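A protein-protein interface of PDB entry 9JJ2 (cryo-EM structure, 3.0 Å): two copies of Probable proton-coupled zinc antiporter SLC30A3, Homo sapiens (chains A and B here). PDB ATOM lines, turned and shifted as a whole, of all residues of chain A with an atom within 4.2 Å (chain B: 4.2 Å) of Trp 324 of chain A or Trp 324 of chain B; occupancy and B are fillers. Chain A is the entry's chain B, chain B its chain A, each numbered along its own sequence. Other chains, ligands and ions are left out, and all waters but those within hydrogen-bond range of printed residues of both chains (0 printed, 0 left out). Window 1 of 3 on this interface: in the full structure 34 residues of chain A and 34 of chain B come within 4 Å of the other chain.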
ATOM      1  N   PHE A 136      -5.373  -5.472 -12.809  1.00  0.00           N
ATOM      2  CA  PHE A 136      -4.482  -6.616 -12.937  1.00  0.00           C
ATOM      3  C   PHE A 136      -5.221  -7.938 -13.069  1.00  0.00           C
ATOM      4  O   PHE A 136      -4.603  -8.937 -13.448  1.00  0.00           O
ATOM      5  CB  PHE A 136      -3.540  -6.687 -11.732  1.00  0.00           C
ATOM      6  CG  PHE A 136      -2.345  -5.796 -11.849  1.00  0.00           C
ATOM      7  CD1 PHE A 136      -1.333  -6.087 -12.741  1.00  0.00           C
ATOM      8  CD2 PHE A 136      -2.236  -4.663 -11.068  1.00  0.00           C
ATOM      9  CE1 PHE A 136      -0.236  -5.267 -12.850  1.00  0.00           C
ATOM     10  CE2 PHE A 136      -1.142  -3.842 -11.174  1.00  0.00           C
ATOM     11  CZ  PHE A 136      -0.140  -4.144 -12.066  1.00  0.00           C
ATOM     12  N   GLU A 294       4.754  -7.162  -1.421  1.00  0.00           N
ATOM     13  CA  GLU A 294       5.219  -6.770  -2.752  1.00  0.00           C
ATOM     14  C   GLU A 294       6.742  -6.684  -2.809  1.00  0.00           C
ATOM     15  O   GLU A 294       7.314  -5.681  -3.235  1.00  0.00           O
ATOM     16  CB  GLU A 294       4.581  -5.453  -3.199  1.00  0.00           C
ATOM     17  CG  GLU A 294       3.179  -5.608  -3.722  1.00  0.00           C
ATOM     18  CD  GLU A 294       2.889  -4.667  -4.860  1.00  0.00           C
ATOM     19  OE1 GLU A 294       3.243  -3.479  -4.753  1.00  0.00           O
ATOM     20  OE2 GLU A 294       2.307  -5.117  -5.865  1.00  0.00           O
ATOM     21  N   GLY A 295       7.398  -7.753  -2.369  1.00  0.00           N
ATOM     22  CA  GLY A 295       8.818  -7.908  -2.581  1.00  0.00           C
ATOM     23  C   GLY A 295       9.109  -8.592  -3.901  1.00  0.00           C
ATOM     24  O   GLY A 295       8.213  -8.995  -4.640  1.00  0.00           O
ATOM     25  N   PRO A 297       9.970 -11.518  -6.388  1.00  0.00           N
ATOM     26  CA  PRO A 297       9.638 -12.945  -6.338  1.00  0.00           C
ATOM     27  C   PRO A 297      10.852 -13.785  -5.970  1.00  0.00           C
ATOM     28  O   PRO A 297      11.999 -13.392  -6.193  1.00  0.00           O
ATOM     29  CB  PRO A 297       9.153 -13.250  -7.760  1.00  0.00           C
ATOM     30  CG  PRO A 297       9.602 -12.096  -8.591  1.00  0.00           C
ATOM     31  CD  PRO A 297       9.619 -10.920  -7.684  1.00  0.00           C
ATOM     32  N   HIS A 322      11.323  -1.908 -10.561  1.00  0.00           N
ATOM     33  CA  HIS A 322      10.329  -2.471  -9.657  1.00  0.00           C
ATOM     34  C   HIS A 322      10.037  -3.900 -10.081  1.00  0.00           C
ATOM     35  O   HIS A 322       9.650  -4.143 -11.227  1.00  0.00           O
ATOM     36  CB  HIS A 322       9.042  -1.649  -9.674  1.00  0.00           C
ATOM     37  CG  HIS A 322       9.179  -0.294  -9.058  1.00  0.00           C
ATOM     38  ND1 HIS A 322       9.362  -0.106  -7.707  1.00  0.00           N
ATOM     39  CD2 HIS A 322       9.153   0.941  -9.611  1.00  0.00           C
ATOM     40  CE1 HIS A 322       9.446   1.187  -7.452  1.00  0.00           C
ATOM     41  NE2 HIS A 322       9.324   1.844  -8.590  1.00  0.00           N
ATOM     42  N   LEU A 323      10.216  -4.841  -9.161  1.00  0.00           N
ATOM     43  CA  LEU A 323       9.893  -6.239  -9.402  1.00  0.00           C
ATOM     44  C   LEU A 323       8.971  -6.720  -8.296  1.00  0.00           C
ATOM     45  O   LEU A 323       9.284  -6.561  -7.114  1.00  0.00           O
ATOM     46  CB  LEU A 323      11.153  -7.104  -9.455  1.00  0.00           C
ATOM     47  CG  LEU A 323      12.315  -6.554 -10.278  1.00  0.00           C
ATOM     48  CD1 LEU A 323      13.565  -7.367 -10.041  1.00  0.00           C
ATOM     49  CD2 LEU A 323      11.960  -6.544 -11.746  1.00  0.00           C
ATOM     50  N   TRP A 324       7.835  -7.291  -8.678  1.00  0.00           N
ATOM     51  CA  TRP A 324       6.892  -7.814  -7.702  1.00  0.00           C
ATOM     52  C   TRP A 324       6.055  -8.887  -8.373  1.00  0.00           C
ATOM     53  O   TRP A 324       6.026  -8.998  -9.600  1.00  0.00           O
ATOM     54  CB  TRP A 324       6.013  -6.704  -7.116  1.00  0.00           C
ATOM     55  CG  TRP A 324       4.961  -6.177  -8.034  1.00  0.00           C
ATOM     56  CD1 TRP A 324       3.650  -6.536  -8.063  1.00  0.00           C
ATOM     57  CD2 TRP A 324       5.127  -5.188  -9.053  1.00  0.00           C
ATOM     58  NE1 TRP A 324       2.986  -5.832  -9.033  1.00  0.00           N
ATOM     59  CE2 TRP A 324       3.873  -4.998  -9.658  1.00  0.00           C
ATOM     60  CE3 TRP A 324       6.215  -4.447  -9.515  1.00  0.00           C
ATOM     61  CZ2 TRP A 324       3.677  -4.100 -10.696  1.00  0.00           C
ATOM     62  CZ3 TRP A 324       6.018  -3.556 -10.544  1.00  0.00           C
ATOM     63  CH2 TRP A 324       4.761  -3.390 -11.125  1.00  0.00           C
ATOM     64  N   ALA A 325       5.383  -9.685  -7.552  1.00  0.00           N
ATOM     65  CA  ALA A 325       4.620 -10.829  -8.026  1.00  0.00           C
ATOM     66  C   ALA A 325       3.179 -10.720  -7.556  1.00  0.00           C
ATOM     67  O   ALA A 325       2.926 -10.509  -6.366  1.00  0.00           O
ATOM     68  CB  ALA A 325       5.232 -12.139  -7.532  1.00  0.00           C
ATOM     69  N   HIS A 331       4.431 -12.694 -12.441  1.00  0.00           N
ATOM     70  CA  HIS A 331       5.452 -11.713 -12.110  1.00  0.00           C
ATOM     71  C   HIS A 331       5.297 -10.493 -13.002  1.00  0.00           C
ATOM     72  O   HIS A 331       4.984 -10.618 -14.188  1.00  0.00           O
ATOM     73  CB  HIS A 331       6.855 -12.294 -12.273  1.00  0.00           C
ATOM     74  CG  HIS A 331       7.136 -13.462 -11.383  1.00  0.00           C
ATOM     75  ND1 HIS A 331       6.392 -13.736 -10.257  1.00  0.00           N
ATOM     76  CD2 HIS A 331       8.082 -14.426 -11.452  1.00  0.00           C
ATOM     77  CE1 HIS A 331       6.865 -14.820  -9.672  1.00  0.00           C
ATOM     78  NE2 HIS A 331       7.892 -15.258 -10.376  1.00  0.00           N
ATOM     79  N   VAL A 332       5.521  -9.312 -12.424  1.00  0.00           N
ATOM     80  CA  VAL A 332       5.431  -8.045 -13.136  1.00  0.00           C
ATOM     81  C   VAL A 332       6.731  -7.286 -12.917  1.00  0.00           C
ATOM     82  O   VAL A 332       7.450  -7.510 -11.943  1.00  0.00           O
ATOM     83  CB  VAL A 332       4.225  -7.201 -12.673  1.00  0.00           C
ATOM     84  CG1 VAL A 332       3.846  -6.183 -13.728  1.00  0.00           C
ATOM     85  CG2 VAL A 332       3.042  -8.089 -12.348  1.00  0.00           C
ATOM     86  N   SER A 334       8.891  -3.282 -13.932  1.00  0.00           N
ATOM     87  CA  SER A 334       8.890  -1.923 -14.454  1.00  0.00           C
ATOM     88  C   SER A 334      10.306  -1.377 -14.368  1.00  0.00           C
ATOM     89  O   SER A 334      11.120  -1.847 -13.573  1.00  0.00           O
ATOM     90  CB  SER A 334       7.928  -1.017 -13.684  1.00  0.00           C
ATOM     91  OG  SER A 334       6.673  -1.643 -13.502  1.00  0.00           O
ATOM     92  N   PHE B 136       9.433  -1.559  -3.584  1.00  0.00           N
ATOM     93  CA  PHE B 136       8.465  -0.503  -3.331  1.00  0.00           C
ATOM     94  C   PHE B 136       8.583   0.087  -1.936  1.00  0.00           C
ATOM     95  O   PHE B 136       7.826   1.001  -1.599  1.00  0.00           O
ATOM     96  CB  PHE B 136       7.045  -1.030  -3.540  1.00  0.00           C
ATOM     97  CG  PHE B 136       6.613  -1.045  -4.971  1.00  0.00           C
ATOM     98  CD1 PHE B 136       6.362   0.136  -5.642  1.00  0.00           C
ATOM     99  CD2 PHE B 136       6.459  -2.238  -5.645  1.00  0.00           C
ATOM    100  CE1 PHE B 136       5.965   0.123  -6.957  1.00  0.00           C
ATOM    101  CE2 PHE B 136       6.063  -2.254  -6.958  1.00  0.00           C
ATOM    102  CZ  PHE B 136       5.815  -1.072  -7.616  1.00  0.00           C
ATOM    103  N   GLU B 294      -5.250  -5.500  -5.146  1.00  0.00           N
ATOM    104  CA  GLU B 294      -4.612  -4.627  -6.133  1.00  0.00           C
ATOM    105  C   GLU B 294      -5.634  -4.056  -7.113  1.00  0.00           C
ATOM    106  O   GLU B 294      -5.424  -4.043  -8.326  1.00  0.00           O
ATOM    107  CB  GLU B 294      -3.492  -5.359  -6.875  1.00  0.00           C
ATOM    108  CG  GLU B 294      -2.213  -5.466  -6.086  1.00  0.00           C
ATOM    109  CD  GLU B 294      -1.015  -5.005  -6.871  1.00  0.00           C
ATOM    110  OE1 GLU B 294      -0.896  -5.388  -8.051  1.00  0.00           O
ATOM    111  OE2 GLU B 294      -0.196  -4.254  -6.311  1.00  0.00           O
ATOM    112  N   GLY B 295      -6.750  -3.585  -6.574  1.00  0.00           N
ATOM    113  CA  GLY B 295      -7.712  -2.863  -7.372  1.00  0.00           C
ATOM    114  C   GLY B 295      -7.389  -1.387  -7.452  1.00  0.00           C
ATOM    115  O   GLY B 295      -6.481  -0.888  -6.794  1.00  0.00           O
ATOM    116  N   PRO B 297      -7.552   2.390  -6.607  1.00  0.00           N
ATOM    117  CA  PRO B 297      -7.879   3.081  -5.356  1.00  0.00           C
ATOM    118  C   PRO B 297      -9.227   3.779  -5.445  1.00  0.00           C
ATOM    119  O   PRO B 297      -9.676   4.176  -6.522  1.00  0.00           O
ATOM    120  CB  PRO B 297      -6.734   4.089  -5.198  1.00  0.00           C
ATOM    121  CG  PRO B 297      -6.122   4.199  -6.558  1.00  0.00           C
ATOM    122  CD  PRO B 297      -6.271   2.848  -7.164  1.00  0.00           C
ATOM    123  N   HIS B 322      -2.565   0.419 -15.745  1.00  0.00           N
ATOM    124  CA  HIS B 322      -2.599  -0.258 -14.456  1.00  0.00           C
ATOM    125  C   HIS B 322      -2.626   0.790 -13.355  1.00  0.00           C
ATOM    126  O   HIS B 322      -1.736   1.642 -13.288  1.00  0.00           O
ATOM    127  CB  HIS B 322      -1.389  -1.170 -14.280  1.00  0.00           C
ATOM    128  CG  HIS B 322      -1.397  -2.369 -15.173  1.00  0.00           C
ATOM    129  ND1 HIS B 322      -2.289  -3.406 -15.018  1.00  0.00           N
ATOM    130  CD2 HIS B 322      -0.617  -2.698 -16.229  1.00  0.00           C
ATOM    131  CE1 HIS B 322      -2.061  -4.321 -15.942  1.00  0.00           C
ATOM    132  NE2 HIS B 322      -1.051  -3.916 -16.689  1.00  0.00           N
ATOM    133  N   LEU B 323      -3.636   0.724 -12.497  1.00  0.00           N
ATOM    134  CA  LEU B 323      -3.738   1.607 -11.344  1.00  0.00           C
ATOM    135  C   LEU B 323      -3.914   0.757 -10.099  1.00  0.00           C
ATOM    136  O   LEU B 323      -4.804  -0.095 -10.048  1.00  0.00           O
ATOM    137  CB  LEU B 323      -4.904   2.586 -11.488  1.00  0.00           C
ATOM    138  CG  LEU B 323      -5.048   3.266 -12.848  1.00  0.00           C
ATOM    139  CD1 LEU B 323      -6.367   3.994 -12.940  1.00  0.00           C
ATOM    140  CD2 LEU B 323      -3.898   4.218 -13.082  1.00  0.00           C
ATOM    141  N   TRP B 324      -3.060   0.980  -9.106  1.00  0.00           N
ATOM    142  CA  TRP B 324      -3.153   0.242  -7.856  1.00  0.00           C
ATOM    143  C   TRP B 324      -2.512   1.077  -6.762  1.00  0.00           C
ATOM    144  O   TRP B 324      -1.788   2.036  -7.035  1.00  0.00           O
ATOM    145  CB  TRP B 324      -2.497  -1.138  -7.965  1.00  0.00           C
ATOM    146  CG  TRP B 324      -1.003  -1.134  -7.982  1.00  0.00           C
ATOM    147  CD1 TRP B 324      -0.175  -1.360  -6.928  1.00  0.00           C
ATOM    148  CD2 TRP B 324      -0.159  -0.904  -9.113  1.00  0.00           C
ATOM    149  NE1 TRP B 324       1.133  -1.286  -7.330  1.00  0.00           N
ATOM    150  CE2 TRP B 324       1.169  -1.004  -8.668  1.00  0.00           C
ATOM    151  CE3 TRP B 324      -0.399  -0.619 -10.458  1.00  0.00           C
ATOM    152  CZ2 TRP B 324       2.252  -0.830  -9.518  1.00  0.00           C
ATOM    153  CZ3 TRP B 324       0.676  -0.448 -11.298  1.00  0.00           C
ATOM    154  CH2 TRP B 324       1.986  -0.553 -10.827  1.00  0.00           C
ATOM    155  N   ALA B 325      -2.799   0.711  -5.519  1.00  0.00           N
ATOM    156  CA  ALA B 325      -2.373   1.480  -4.361  1.00  0.00           C
ATOM    157  C   ALA B 325      -1.545   0.609  -3.431  1.00  0.00           C
ATOM    158  O   ALA B 325      -1.966  -0.493  -3.069  1.00  0.00           O
ATOM    159  CB  ALA B 325      -3.577   2.048  -3.609  1.00  0.00           C
ATOM    160  N   HIS B 331      -0.241   5.733  -4.236  1.00  0.00           N
ATOM    161  CA  HIS B 331      -0.823   5.248  -5.477  1.00  0.00           C
ATOM    162  C   HIS B 331       0.260   5.145  -6.539  1.00  0.00           C
ATOM    163  O   HIS B 331       1.164   5.982  -6.598  1.00  0.00           O
ATOM    164  CB  HIS B 331      -1.938   6.169  -5.968  1.00  0.00           C
ATOM    165  CG  HIS B 331      -3.070   6.321  -5.003  1.00  0.00           C
ATOM    166  ND1 HIS B 331      -3.353   5.386  -4.034  1.00  0.00           N
ATOM    167  CD2 HIS B 331      -3.993   7.300  -4.862  1.00  0.00           C
ATOM    168  CE1 HIS B 331      -4.401   5.782  -3.334  1.00  0.00           C
ATOM    169  NE2 HIS B 331      -4.809   6.940  -3.818  1.00  0.00           N
ATOM    170  N   VAL B 332       0.161   4.113  -7.377  1.00  0.00           N
ATOM    171  CA  VAL B 332       1.100   3.875  -8.463  1.00  0.00           C
ATOM    172  C   VAL B 332       0.302   3.714  -9.749  1.00  0.00           C
ATOM    173  O   VAL B 332      -0.879   3.369  -9.733  1.00  0.00           O
ATOM    174  CB  VAL B 332       1.979   2.631  -8.210  1.00  0.00           C
ATOM    175  CG1 VAL B 332       3.233   2.678  -9.058  1.00  0.00           C
ATOM    176  CG2 VAL B 332       2.337   2.517  -6.744  1.00  0.00           C
ATOM    177  N   SER B 334       0.755   2.842 -14.297  1.00  0.00           N
ATOM    178  CA  SER B 334       1.541   2.430 -15.451  1.00  0.00           C
ATOM    179  C   SER B 334       0.664   2.531 -16.686  1.00  0.00           C
ATOM    180  O   SER B 334      -0.564   2.499 -16.600  1.00  0.00           O
ATOM    181  CB  SER B 334       2.077   1.006 -15.296  1.00  0.00           C
ATOM    182  OG  SER B 334       2.624   0.805 -14.008  1.00  0.00           O
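The side-chain carboxylate of Glu 294 of chain A sits close to the side-chain carboxylate of Glu 294 of chain B.
The indole nitrogen (NE1) of Trp 324 of chain B sits close to the side-chain carboxylate (OE2) of Glu 294 of chain B, at 3.4 Å. The backbone carbonyl oxygen (O) of His 322 of chain B lies within hydrogen-bond range of the backbone NH (N) of Ser 334 of chain B (2.9 Å). The backbone NH of Val 332 of chain B is in hydrogen-bond range of the backbone carbonyl oxygen of Trp 324 of chain B, at 2.9 Å. NE1 of Trp 324 of chain A sits close to OE2 of Glu 294 of chain A, 3.3 Å away. The backbone NH (N) of Ser 334 of chain A sits at hydrogen-bond distance from the backbone carbonyl oxygen (O) of His 322 of chain A (2.9 Å). The backbone NH (N) of Val 332 of chain A sits at hydrogen-bond distance from the backbone carbonyl oxygen (O) of Trp 324 of chain A, 2.9 Å away.
Phe 136 of chain A touches Glu 294 of chain B (CD2 to OE1, 3.4 Å). Phe 136 of chain A touches His 322 of chain B. CE2 of Phe 136 of chain A touches CE3 of Trp 324 of chain B (3.4 Å). Glu 294 of chain A touches Phe 136 of chain B. OE1 of Glu 294 of chain A touches NE1 of Trp 324 of chain B, at 3.99 Å. His 322 of chain A touches Phe 136 of chain B (ND1 to CE1, 3.5 Å). Trp 324 of chain A touches Phe 136 of chain B (CE3 to CE2, 3.4 Å). Trp 324 of chain B touches Trp 324 of chain A (CZ2 to CZ2, 3.8 Å).
Printed residues of chain B within 4 Å of Phe 136 of chain A: Glu 294 (3.4 Å), His 322 (3.5 Å) and Trp 324 (3.4 Å). Of the printed residues of chain B, Glu 294 of chain A touches Phe 136, Glu 294 and Trp 324. Printed residues of chain B within 4 Å of His 322 of chain A: Phe 136 (3.5 Å). Trp 324 of chain A touches two residues of chain B. Of the printed residues of chain A, Phe 136 of chain B touches Glu 294 (3.6 Å), His 322 (3.5 Å) and Trp 324 (3.4 Å). Of the printed residues of chain A, Glu 294 of chain B touches Phe 136 (3.4 Å) and Glu 294 (2.7 Å). The nearest residue of chain B that does not touch Trp 324 of chain A is Glu 294 of chain B (4.03 Å). The nearest printed residue of chain A that does not touch Trp 324 of chain B is Ser 334 of chain A (5.5 Å). The nearest printed residue of chain B that does not touch Phe 136 of chain A is Leu 323 of chain B (5.3 Å).
Hydrophobic or aromatic side chains of chain A that line the printed part of chain B: Phe 136, His 322 and Trp 324. Of the 11 printed residues of chain B, 4 touch a printed residue of chain A. Among the printed residues, no Asp or Glu carboxylate lies within 4 Å of a Lys or Arg side-chain nitrogen of the other chain.
Phe 136 of chain A touches His 322 of chain B, and with the chains exchanged His 322 of chain A touches Phe 136 of chain B. Phe 136 of chain A touches Trp 324 of chain B, and with the chains exchanged Trp 324 of chain A touches Phe 136 of chain B. Glu 294 of chain A touches Trp 324 of chain B, but with the chains exchanged Trp 324 of chain A does not touch Glu 294 of chain B (4.03 Å). Trp 324 of chain A touches its own counterpart, Trp 324 of chain B. Positions printed for both chains: 136, 294, 295, 297, 322, 323, 324, 325, 331, 332 and 334. Of the 9 pairs that touch across the chains among the printed residues, 8 have their exchanged pair printed and touching as well.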
